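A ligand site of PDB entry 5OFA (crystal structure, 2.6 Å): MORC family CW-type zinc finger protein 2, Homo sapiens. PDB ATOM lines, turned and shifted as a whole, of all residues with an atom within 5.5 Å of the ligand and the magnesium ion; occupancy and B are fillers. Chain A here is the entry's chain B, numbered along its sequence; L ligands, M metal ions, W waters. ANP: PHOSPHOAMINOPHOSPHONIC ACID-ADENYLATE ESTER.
OD2 of Asp 71 sits at hydrogen-bond distance from N6 of the ligand, 2.7 Å away.
O3G of the ligand is in salt-bridge range of NZ of Lys 430 (2.7 Å).
OG of Ser 90 lies within hydrogen-bond range of O1B of the ligand, at 2.7 Å.
The backbone NH of Asn 105 lies within hydrogen-bond range of an oxygen (O2G) of the ligand.
The side-chain amino group (NZ) of Lys 108 is in salt-bridge range of an oxygen (O1A) of the ligand, 2.9 Å away.
An oxygen (O2G) of the ligand is in hydrogen-bond range of the backbone NH (N) of Gly 106 (2.9 Å).
An oxygen (O3G) of the ligand sits at hydrogen-bond distance from the backbone NH (N) of Gln 102 (2.9 Å).
An oxygen (O2G) of the ligand sits at hydrogen-bond distance from the backbone NH of Gly 104, 2.9 Å away.
An oxygen (O2B) of the ligand sits close to the side-chain amino group (NZ) of Lys 92, 2.9 Å away.
O3G of the ligand is in hydrogen-bond range of N of Tyr 103, at 3.1 Å.
O1A of the ligand sits at hydrogen-bond distance from N of Leu 107.
OG1 of Thr 200 is in hydrogen-bond range of N1 of the ligand (3.4 Å).
NZ of Lys 92 lies close to OD1 of Asn 42 (3.3 Å).
O of Glu 38 lies close to ND2 of Asn 42 (3.4 Å).
The backbone NH (N) of Asp 71 lies within hydrogen-bond range of the backbone carbonyl oxygen (O) of Thr 200 (2.9 Å).
NZ of Lys 430 is in hydrogen-bond range of O of Ile 100.
The backbone carbonyl oxygen of Val 84 sits at hydrogen-bond distance from the side-chain amino group of Lys 108.
NZ of Lys 92 is in salt-bridge range of OD2 of Asp 45.
The side-chain carboxylate of Asp 45 lies within hydrogen-bond range of the backbone NH of Gly 101 (2.9 Å).
The side-chain hydroxyl (OG) of Ser 83 lies within hydrogen-bond range of the side-chain amino group (NZ) of Lys 89 (3.2 Å).
Glu 38 touches the ligand.
CB of Ala 46 touches N1 of the ligand (3.4 Å).
Gly 75 touches the ligand.
Met 76 touches the ligand (CG to N3, 3.6 Å).
CG2 of Val 84 touches O4' of the ligand (3.3 Å).
O of Lys 89 touches O1B of the ligand, 3.97 Å away.
CA of Gly 101 touches O3G of the ligand, 3.3 Å away.
Hydrophobic or aromatic side chains within 4 Å of the ligand: Ala 46, Met 76, Val 84, Tyr 103 and Leu 107.
20 residues have an atom within 4 Å of the ligand: Glu 38, Asn 42, Ala 46, Asp 71, Gly 75, Met 76, Val 84, Lys 89, Ser 90, Lys 92, Gly 101, Gln 102, Tyr 103, Gly 104, Asn 105, Gly 106, Leu 107, Lys 108, Thr 200 and Lys 430.
The nearest printed residue that does not touch the ligand is Ala 43 (4.1 Å).
Lys 92 touches the magnesium ion.
The nearest printed residue that does not touch the magnesium ion is Glu 38 (4.01 Å).
An oxygen (O1G) of the ligand binds the magnesium ion.
OD1 of Asn 42 binds the magnesium ion, at 2.0 Å.
Water W1 binds the magnesium ion, 2.2 Å away.
The magnesium ion is bound by an oxygen (O2B) of the ligand.
The magnesium ion is bound by O2A of the ligand (2.3 Å).
The magnesium ion has five donor atoms within binding distance.
Water W1 bridges OE2 of Glu 38 (2.6 Å) and ND2 of Asn 42 (3.2 Å).
Water W2 lies within hydrogen-bond range of O2G of the ligand (2.7 Å), N of Gly 106 (3.2 Å) and OE1 of Glu 38 (3.3 Å).
Water W3 lies within hydrogen-bond range of OD1 of Asp 71 (2.5 Å), N1 of the ligand (2.8 Å), OG1 of Thr 200 (2.9 Å) and N of Gly 75 (3.1 Å).
Water W4 lies within hydrogen-bond range of O of Leu 39 (2.7 Å) and N6 of the ligand (3.1 Å).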
ATOM      1  N   GLU A  38      19.510  12.962  10.618  1.00  0.00           N
ATOM      2  CA  GLU A  38      18.568  11.866  10.430  1.00  0.00           C
ATOM      3  C   GLU A  38      17.199  12.268  10.963  1.00  0.00           C
ATOM      4  O   GLU A  38      16.155  11.900  10.346  1.00  0.00           O
ATOM      5  CB  GLU A  38      19.037  10.578  11.101  1.00  0.00           C
ATOM      6  CG  GLU A  38      20.264   9.944  10.433  1.00  0.00           C
ATOM      7  CD  GLU A  38      19.987   9.131   9.151  1.00  0.00           C
ATOM      8  OE1 GLU A  38      20.999   8.414   8.747  1.00  0.00           O
ATOM      9  OE2 GLU A  38      18.803   9.147   8.577  1.00  0.00           O
ATOM     10  N   LEU A  39      17.151  12.971  12.090  1.00  0.00           N
ATOM     11  CA  LEU A  39      15.823  13.294  12.684  1.00  0.00           C
ATOM     12  C   LEU A  39      15.144  14.436  11.940  1.00  0.00           C
ATOM     13  O   LEU A  39      13.897  14.452  11.794  1.00  0.00           O
ATOM     14  CB  LEU A  39      15.960  13.618  14.167  1.00  0.00           C
ATOM     15  CG  LEU A  39      16.167  12.331  15.021  1.00  0.00           C
ATOM     16  CD1 LEU A  39      17.582  11.799  14.933  1.00  0.00           C
ATOM     17  CD2 LEU A  39      15.785  12.597  16.466  1.00  0.00           C
ATOM     18  N   ASP A  41      15.623  14.928   8.684  1.00  0.00           N
ATOM     19  CA  ASP A  41      15.191  14.251   7.448  1.00  0.00           C
ATOM     20  C   ASP A  41      13.819  13.609   7.644  1.00  0.00           C
ATOM     21  O   ASP A  41      12.958  13.655   6.754  1.00  0.00           O
ATOM     22  CB  ASP A  41      16.129  13.135   7.014  1.00  0.00           C
ATOM     23  CG  ASP A  41      17.529  13.609   6.576  1.00  0.00           C
ATOM     24  OD1 ASP A  41      17.716  14.800   6.221  1.00  0.00           O
ATOM     25  OD2 ASP A  41      18.451  12.713   6.558  1.00  0.00           O
ATOM     26  N   ASN A  42      13.604  12.992   8.807  1.00  0.00           N
ATOM     27  CA  ASN A  42      12.368  12.324   9.022  1.00  0.00           C
ATOM     28  C   ASN A  42      11.199  13.346   9.089  1.00  0.00           C
ATOM     29  O   ASN A  42      10.095  13.063   8.598  1.00  0.00           O
ATOM     30  CB  ASN A  42      12.394  11.469  10.272  1.00  0.00           C
ATOM     31  CG  ASN A  42      13.246  10.221  10.121  1.00  0.00           C
ATOM     32  OD1 ASN A  42      13.505   9.755   9.013  1.00  0.00           O
ATOM     33  ND2 ASN A  42      13.718   9.673  11.255  1.00  0.00           N
ATOM     34  N   ALA A  43      11.433  14.499   9.691  1.00  0.00           N
ATOM     35  CA  ALA A  43      10.408  15.545   9.725  1.00  0.00           C
ATOM     36  C   ALA A  43      10.112  16.068   8.318  1.00  0.00           C
ATOM     37  O   ALA A  43       8.976  16.252   7.958  1.00  0.00           O
ATOM     38  CB  ALA A  43      10.828  16.677  10.624  1.00  0.00           C
ATOM     39  N   ASP A  45      10.480  14.448   5.451  1.00  0.00           N
ATOM     40  CA  ASP A  45       9.787  13.337   4.817  1.00  0.00           C
ATOM     41  C   ASP A  45       8.301  13.214   5.287  1.00  0.00           C
ATOM     42  O   ASP A  45       7.483  12.791   4.514  1.00  0.00           O
ATOM     43  CB  ASP A  45      10.519  12.028   5.118  1.00  0.00           C
ATOM     44  CG  ASP A  45      11.842  11.828   4.321  1.00  0.00           C
ATOM     45  OD1 ASP A  45      12.117  12.530   3.298  1.00  0.00           O
ATOM     46  OD2 ASP A  45      12.563  10.855   4.726  1.00  0.00           O
ATOM     47  N   ALA A  46       7.982  13.577   6.532  1.00  0.00           N
ATOM     48  CA  ALA A  46       6.625  13.532   7.019  1.00  0.00           C
ATOM     49  C   ALA A  46       5.829  14.796   6.652  1.00  0.00           C
ATOM     50  O   ALA A  46       4.769  15.062   7.233  1.00  0.00           O
ATOM     51  CB  ALA A  46       6.660  13.364   8.543  1.00  0.00           C
ATOM     52  N   ASP A  71       8.016  18.487  15.335  1.00  0.00           N
ATOM     53  CA  ASP A  71       7.568  18.810  13.990  1.00  0.00           C
ATOM     54  C   ASP A  71       6.053  18.744  13.894  1.00  0.00           C
ATOM     55  O   ASP A  71       5.381  18.115  14.717  1.00  0.00           O
ATOM     56  CB  ASP A  71       8.230  17.903  12.945  1.00  0.00           C
ATOM     57  CG  ASP A  71       7.675  16.467  12.930  1.00  0.00           C
ATOM     58  OD1 ASP A  71       6.449  16.301  12.689  1.00  0.00           O
ATOM     59  OD2 ASP A  71       8.454  15.482  13.130  1.00  0.00           O
ATOM     60  N   ALA A  74       3.082  14.673   9.414  1.00  0.00           N
ATOM     61  CA  ALA A  74       1.941  13.773   9.371  1.00  0.00           C
ATOM     62  C   ALA A  74       1.711  12.905  10.601  1.00  0.00           C
ATOM     63  O   ALA A  74       0.615  12.294  10.752  1.00  0.00           O
ATOM     64  CB  ALA A  74       2.063  12.867   8.142  1.00  0.00           C
ATOM     65  N   GLY A  75       2.729  12.778  11.448  1.00  0.00           N
ATOM     66  CA  GLY A  75       2.639  11.916  12.620  1.00  0.00           C
ATOM     67  C   GLY A  75       2.546  10.438  12.258  1.00  0.00           C
ATOM     68  O   GLY A  75       2.760  10.032  11.097  1.00  0.00           O
ATOM     69  N   MET A  76       2.249   9.640  13.264  1.00  0.00           N
ATOM     70  CA  MET A  76       2.231   8.192  13.133  1.00  0.00           C
ATOM     71  C   MET A  76       1.066   7.628  13.924  1.00  0.00           C
ATOM     72  O   MET A  76       0.854   7.987  15.068  1.00  0.00           O
ATOM     73  CB  MET A  76       3.518   7.597  13.683  1.00  0.00           C
ATOM     74  CG  MET A  76       4.754   7.735  12.803  1.00  0.00           C
ATOM     75  SD  MET A  76       6.248   7.075  13.628  1.00  0.00           S
ATOM     76  CE  MET A  76       6.713   8.433  14.722  1.00  0.00           C
ATOM     77  N   ASP A  80       2.225   2.487  12.379  1.00  0.00           N
ATOM     78  CA  ASP A  80       3.398   3.230  11.916  1.00  0.00           C
ATOM     79  C   ASP A  80       4.445   3.343  13.020  1.00  0.00           C
ATOM     80  O   ASP A  80       5.636   3.201  12.767  1.00  0.00           O
ATOM     81  CB  ASP A  80       3.072   4.673  11.525  1.00  0.00           C
ATOM     82  CG  ASP A  80       2.030   4.809  10.389  1.00  0.00           C
ATOM     83  OD1 ASP A  80       2.080   3.954   9.475  1.00  0.00           O
ATOM     84  OD2 ASP A  80       1.182   5.788  10.414  1.00  0.00           O
ATOM     85  N   SER A  83       6.251   0.098  13.566  1.00  0.00           N
ATOM     86  CA  SER A  83       7.188  -0.226  12.505  1.00  0.00           C
ATOM     87  C   SER A  83       8.514   0.517  12.665  1.00  0.00           C
ATOM     88  O   SER A  83       9.466   0.081  12.061  1.00  0.00           O
ATOM     89  CB  SER A  83       6.678   0.107  11.096  1.00  0.00           C
ATOM     90  OG  SER A  83       5.575  -0.592  10.714  1.00  0.00           O
ATOM     91  N   VAL A  84       8.570   1.606  13.452  1.00  0.00           N
ATOM     92  CA  VAL A  84       9.831   2.276  13.750  1.00  0.00           C
ATOM     93  C   VAL A  84      10.888   1.268  14.237  1.00  0.00           C
ATOM     94  O   VAL A  84      12.081   1.320  13.841  1.00  0.00           O
ATOM     95  CB  VAL A  84       9.655   3.383  14.793  1.00  0.00           C
ATOM     96  CG1 VAL A  84      10.991   3.945  15.251  1.00  0.00           C
ATOM     97  CG2 VAL A  84       8.817   4.515  14.221  1.00  0.00           C
ATOM     98  N   LYS A  89      12.649  -1.444   7.857  1.00  0.00           N
ATOM     99  CA  LYS A  89      11.337  -1.202   7.325  1.00  0.00           C
ATOM    100  C   LYS A  89      11.192   0.279   7.029  1.00  0.00           C
ATOM    101  O   LYS A  89      11.435   1.125   7.895  1.00  0.00           O
ATOM    102  CB  LYS A  89      10.285  -1.626   8.323  1.00  0.00           C
ATOM    103  CG  LYS A  89       8.872  -1.646   7.742  1.00  0.00           C
ATOM    104  CD  LYS A  89       7.973  -2.585   8.563  1.00  0.00           C
ATOM    105  CE  LYS A  89       6.487  -2.426   8.221  1.00  0.00           C
ATOM    106  NZ  LYS A  89       5.680  -3.344   9.078  1.00  0.00           N
ATOM    107  N   SER A  90      10.832   0.578   5.789  1.00  0.00           N
ATOM    108  CA  SER A  90      10.619   1.937   5.345  1.00  0.00           C
ATOM    109  C   SER A  90       9.553   1.898   4.253  1.00  0.00           C
ATOM    110  O   SER A  90       9.790   1.348   3.168  1.00  0.00           O
ATOM    111  CB  SER A  90      11.935   2.553   4.803  1.00  0.00           C
ATOM    112  OG  SER A  90      11.726   3.927   4.484  1.00  0.00           O
ATOM    113  N   ALA A  91       8.371   2.455   4.536  1.00  0.00           N
ATOM    114  CA  ALA A  91       7.322   2.691   3.497  1.00  0.00           C
ATOM    115  C   ALA A  91       7.730   3.717   2.451  1.00  0.00           C
ATOM    116  O   ALA A  91       7.096   3.836   1.405  1.00  0.00           O
ATOM    117  CB  ALA A  91       6.022   3.131   4.141  1.00  0.00           C
ATOM    118  N   LYS A  92       8.818   4.447   2.728  1.00  0.00           N
ATOM    119  CA  LYS A  92       9.413   5.406   1.779  1.00  0.00           C
ATOM    120  C   LYS A  92      10.177   4.754   0.643  1.00  0.00           C
ATOM    121  O   LYS A  92      10.374   5.392  -0.392  1.00  0.00           O
ATOM    122  CB  LYS A  92      10.381   6.341   2.503  1.00  0.00           C
ATOM    123  CG  LYS A  92       9.799   7.022   3.736  1.00  0.00           C
ATOM    124  CD  LYS A  92      10.857   7.826   4.451  1.00  0.00           C
ATOM    125  CE  LYS A  92      10.319   8.318   5.770  1.00  0.00           C
ATOM    126  NZ  LYS A  92      11.385   9.019   6.528  1.00  0.00           N
ATOM    127  N   ILE A 100      13.768  11.196   1.387  1.00  0.00           N
ATOM    128  CA  ILE A 100      15.154  10.979   1.720  1.00  0.00           C
ATOM    129  C   ILE A 100      15.344   9.584   2.355  1.00  0.00           C
ATOM    130  O   ILE A 100      16.254   8.854   1.991  1.00  0.00           O
ATOM    131  CB  ILE A 100      15.642  12.098   2.629  1.00  0.00           C
ATOM    132  CG1 ILE A 100      15.592  13.427   1.830  1.00  0.00           C
ATOM    133  CG2 ILE A 100      17.027  11.775   3.116  1.00  0.00           C
ATOM    134  CD1 ILE A 100      15.526  14.634   2.725  1.00  0.00           C
ATOM    135  N   GLY A 101      14.431   9.202   3.239  1.00  0.00           N
ATOM    136  CA  GLY A 101      14.530   7.924   3.911  1.00  0.00           C
ATOM    137  C   GLY A 101      14.357   6.754   2.975  1.00  0.00           C
ATOM    138  O   GLY A 101      13.505   6.775   2.102  1.00  0.00           O
ATOM    139  N   GLN A 102      15.212   5.743   3.133  1.00  0.00           N
ATOM    140  CA  GLN A 102      15.095   4.552   2.374  1.00  0.00           C
ATOM    141  C   GLN A 102      15.649   3.327   3.080  1.00  0.00           C
ATOM    142  O   GLN A 102      15.318   2.242   2.685  1.00  0.00           O
ATOM    143  CB  GLN A 102      15.796   4.731   1.025  1.00  0.00           C
ATOM    144  CG  GLN A 102      17.287   5.052   1.029  1.00  0.00           C
ATOM    145  CD  GLN A 102      17.959   5.049  -0.370  1.00  0.00           C
ATOM    146  OE1 GLN A 102      18.667   5.976  -0.740  1.00  0.00           O
ATOM    147  NE2 GLN A 102      17.724   3.974  -1.150  1.00  0.00           N
ATOM    148  N   TYR A 103      16.469   3.470   4.143  1.00  0.00           N
ATOM    149  CA  TYR A 103      17.148   2.331   4.745  1.00  0.00           C
ATOM    150  C   TYR A 103      16.496   1.785   6.034  1.00  0.00           C
ATOM    151  O   TYR A 103      16.888   0.702   6.513  1.00  0.00           O
ATOM    152  CB  TYR A 103      18.633   2.677   4.991  1.00  0.00           C
ATOM    153  CG  TYR A 103      19.531   2.904   3.762  1.00  0.00           C
ATOM    154  CD1 TYR A 103      19.296   2.277   2.537  1.00  0.00           C
ATOM    155  CD2 TYR A 103      20.648   3.781   3.819  1.00  0.00           C
ATOM    156  CE1 TYR A 103      20.147   2.483   1.424  1.00  0.00           C
ATOM    157  CE2 TYR A 103      21.510   3.979   2.706  1.00  0.00           C
ATOM    158  CZ  TYR A 103      21.257   3.313   1.509  1.00  0.00           C
ATOM    159  OH  TYR A 103      22.075   3.495   0.413  1.00  0.00           O
ATOM    160  N   GLY A 104      15.521   2.465   6.615  1.00  0.00           N
ATOM    161  CA  GLY A 104      14.816   1.893   7.784  1.00  0.00           C
ATOM    162  C   GLY A 104      15.645   1.857   9.069  1.00  0.00           C
ATOM    163  O   GLY A 104      15.451   1.024   9.942  1.00  0.00           O
ATOM    164  N   ASN A 105      16.587   2.778   9.165  1.00  0.00           N
ATOM    165  CA  ASN A 105      17.577   2.807  10.247  1.00  0.00           C
ATOM    166  C   ASN A 105      17.879   4.172  10.901  1.00  0.00           C
ATOM    167  O   ASN A 105      18.250   4.194  12.060  1.00  0.00           O
ATOM    168  CB  ASN A 105      18.842   2.277   9.653  1.00  0.00           C
ATOM    169  CG  ASN A 105      19.841   1.790  10.713  1.00  0.00           C
ATOM    170  OD1 ASN A 105      19.481   1.151  11.691  1.00  0.00           O
ATOM    171  ND2 ASN A 105      21.107   2.049  10.457  1.00  0.00           N
ATOM    172  N   GLY A 106      17.687   5.289  10.187  1.00  0.00           N
ATOM    173  CA  GLY A 106      18.239   6.588  10.586  1.00  0.00           C
ATOM    174  C   GLY A 106      17.916   7.068  11.986  1.00  0.00           C
ATOM    175  O   GLY A 106      18.796   7.482  12.714  1.00  0.00           O
ATOM    176  N   LEU A 107      16.674   6.953  12.394  1.00  0.00           N
ATOM    177  CA  LEU A 107      16.283   7.411  13.732  1.00  0.00           C
ATOM    178  C   LEU A 107      17.054   6.623  14.788  1.00  0.00           C
ATOM    179  O   LEU A 107      17.504   7.180  15.811  1.00  0.00           O
ATOM    180  CB  LEU A 107      14.777   7.288  13.957  1.00  0.00           C
ATOM    181  CG  LEU A 107      14.258   7.479  15.363  1.00  0.00           C
ATOM    182  CD1 LEU A 107      14.579   8.848  15.978  1.00  0.00           C
ATOM    183  CD2 LEU A 107      12.759   7.307  15.408  1.00  0.00           C
ATOM    184  N   LYS A 108      17.213   5.326  14.552  1.00  0.00           N
ATOM    185  CA  LYS A 108      17.892   4.480  15.553  1.00  0.00           C
ATOM    186  C   LYS A 108      19.419   4.679  15.546  1.00  0.00           C
ATOM    187  O   LYS A 108      20.015   4.769  16.606  1.00  0.00           O
ATOM    188  CB  LYS A 108      17.550   3.022  15.320  1.00  0.00           C
ATOM    189  CG  LYS A 108      16.083   2.691  15.639  1.00  0.00           C
ATOM    190  CD  LYS A 108      15.096   2.971  14.516  1.00  0.00           C
ATOM    191  CE  LYS A 108      15.279   2.054  13.309  1.00  0.00           C
ATOM    192  NZ  LYS A 108      14.214   2.243  12.268  1.00  0.00           N
ATOM    193  N   LEU A 120       9.758   9.176  22.292  1.00  0.00           N
ATOM    194  CA  LEU A 120       9.105   9.810  21.161  1.00  0.00           C
ATOM    195  C   LEU A 120       7.588   9.860  21.439  1.00  0.00           C
ATOM    196  O   LEU A 120       7.012   8.886  21.944  1.00  0.00           O
ATOM    197  CB  LEU A 120       9.444   9.010  19.898  1.00  0.00           C
ATOM    198  CG  LEU A 120       8.748   9.308  18.557  1.00  0.00           C
ATOM    199  CD1 LEU A 120       9.655   8.802  17.445  1.00  0.00           C
ATOM    200  CD2 LEU A 120       7.343   8.686  18.440  1.00  0.00           C
ATOM    201  N   THR A 200       5.010  15.029  15.610  1.00  0.00           N
ATOM    202  CA  THR A 200       5.892  14.136  16.350  1.00  0.00           C
ATOM    203  C   THR A 200       6.886  14.943  17.166  1.00  0.00           C
ATOM    204  O   THR A 200       7.394  15.979  16.711  1.00  0.00           O
ATOM    205  CB  THR A 200       6.652  13.221  15.382  1.00  0.00           C
ATOM    206  OG1 THR A 200       5.709  12.501  14.567  1.00  0.00           O
ATOM    207  CG2 THR A 200       7.554  12.256  16.152  1.00  0.00           C
ATOM    208  N   VAL A 202      10.402  14.065  19.296  1.00  0.00           N
ATOM    209  CA  VAL A 202      11.440  13.107  19.674  1.00  0.00           C
ATOM    210  C   VAL A 202      12.329  13.769  20.705  1.00  0.00           C
ATOM    211  O   VAL A 202      12.842  14.857  20.469  1.00  0.00           O
ATOM    212  CB  VAL A 202      12.264  12.683  18.467  1.00  0.00           C
ATOM    213  CG1 VAL A 202      13.248  11.569  18.867  1.00  0.00           C
ATOM    214  CG2 VAL A 202      11.409  12.224  17.336  1.00  0.00           C
ATOM    215  N   LYS A 430      24.778   8.328   5.587  1.00  0.00           N
ATOM    216  CA  LYS A 430      24.392   9.440   4.717  1.00  0.00           C
ATOM    217  C   LYS A 430      25.361  10.592   4.738  1.00  0.00           C
ATOM    218  O   LYS A 430      24.938  11.735   4.647  1.00  0.00           O
ATOM    219  CB  LYS A 430      22.976   9.892   4.973  1.00  0.00           C
ATOM    220  CG  LYS A 430      22.045   8.723   4.786  1.00  0.00           C
ATOM    221  CD  LYS A 430      20.653   9.097   4.370  1.00  0.00           C
ATOM    222  CE  LYS A 430      19.763   7.857   4.500  1.00  0.00           C
ATOM    223  NZ  LYS A 430      18.381   8.245   4.163  1.00  0.00           N
HETATM  224  PG  ANP L   1      16.379   6.034   6.761  1.00  0.00           P
HETATM  225  O1G ANP L   1      16.031   7.114   7.779  1.00  0.00           O
HETATM  226  O2G ANP L   1      17.028   4.825   7.405  1.00  0.00           O
HETATM  227  O3G ANP L   1      16.975   6.273   5.373  1.00  0.00           O
HETATM  228  PB  ANP L   1      13.510   5.721   7.448  1.00  0.00           P
HETATM  229  O1B ANP L   1      12.328   4.880   6.972  1.00  0.00           O
HETATM  230  O2B ANP L   1      13.156   7.131   7.868  1.00  0.00           O
HETATM  231  N3B ANP L   1      14.731   5.592   6.273  1.00  0.00           N
HETATM  232  PA  ANP L   1      13.937   5.831  10.191  1.00  0.00           P
HETATM  233  O1A ANP L   1      14.467   4.917  11.262  1.00  0.00           O
HETATM  234  O2A ANP L   1      14.569   7.249   9.889  1.00  0.00           O
HETATM  235  O3A ANP L   1      14.119   5.043   8.799  1.00  0.00           O
HETATM  236  O5' ANP L   1      12.398   5.912  10.518  1.00  0.00           O
HETATM  237  C5' ANP L   1      11.585   4.767  10.315  1.00  0.00           C
HETATM  238  C4' ANP L   1      10.135   5.213  10.203  1.00  0.00           C
HETATM  239  O4' ANP L   1       9.677   5.940  11.346  1.00  0.00           O
HETATM  240  C3' ANP L   1       9.988   6.202   9.077  1.00  0.00           C
HETATM  241  O3' ANP L   1       9.963   5.484   7.842  1.00  0.00           O
HETATM  242  C2' ANP L   1       8.731   6.925   9.441  1.00  0.00           C
HETATM  243  O2' ANP L   1       7.644   6.084   9.039  1.00  0.00           O
HETATM  244  C1' ANP L   1       8.756   6.971  10.937  1.00  0.00           C
HETATM  245  N9  ANP L   1       9.156   8.295  11.440  1.00  0.00           N
HETATM  246  C8  ANP L   1      10.310   8.624  12.054  1.00  0.00           C
HETATM  247  N7  ANP L   1      10.308   9.938  12.442  1.00  0.00           N
HETATM  248  C5  ANP L   1       9.134  10.481  12.066  1.00  0.00           C
HETATM  249  C6  ANP L   1       8.494  11.818  12.125  1.00  0.00           C
HETATM  250  N6  ANP L   1       9.061  12.895  12.671  1.00  0.00           N
HETATM  251  N1  ANP L   1       7.258  11.933  11.606  1.00  0.00           N
HETATM  252  C2  ANP L   1       6.652  10.873  11.042  1.00  0.00           C
HETATM  253  N3  ANP L   1       7.167   9.630  10.928  1.00  0.00           N
HETATM  254  C4  ANP L   1       8.385   9.376  11.422  1.00  0.00           C
HETATM  255 MG    MG M   1      14.859   8.632   8.057  1.00  0.00          MG
HETATM  256  O   HOH W   1      16.407   9.427   9.457  1.00  0.00           O
HETATM  257  O   HOH W   2      19.631   5.647   7.682  1.00  0.00           O
HETATM  258  O   HOH W   3       5.505  14.026  12.069  1.00  0.00           O
HETATM  259  O   HOH W   4      11.990  13.596  13.528  1.00  0.00           O
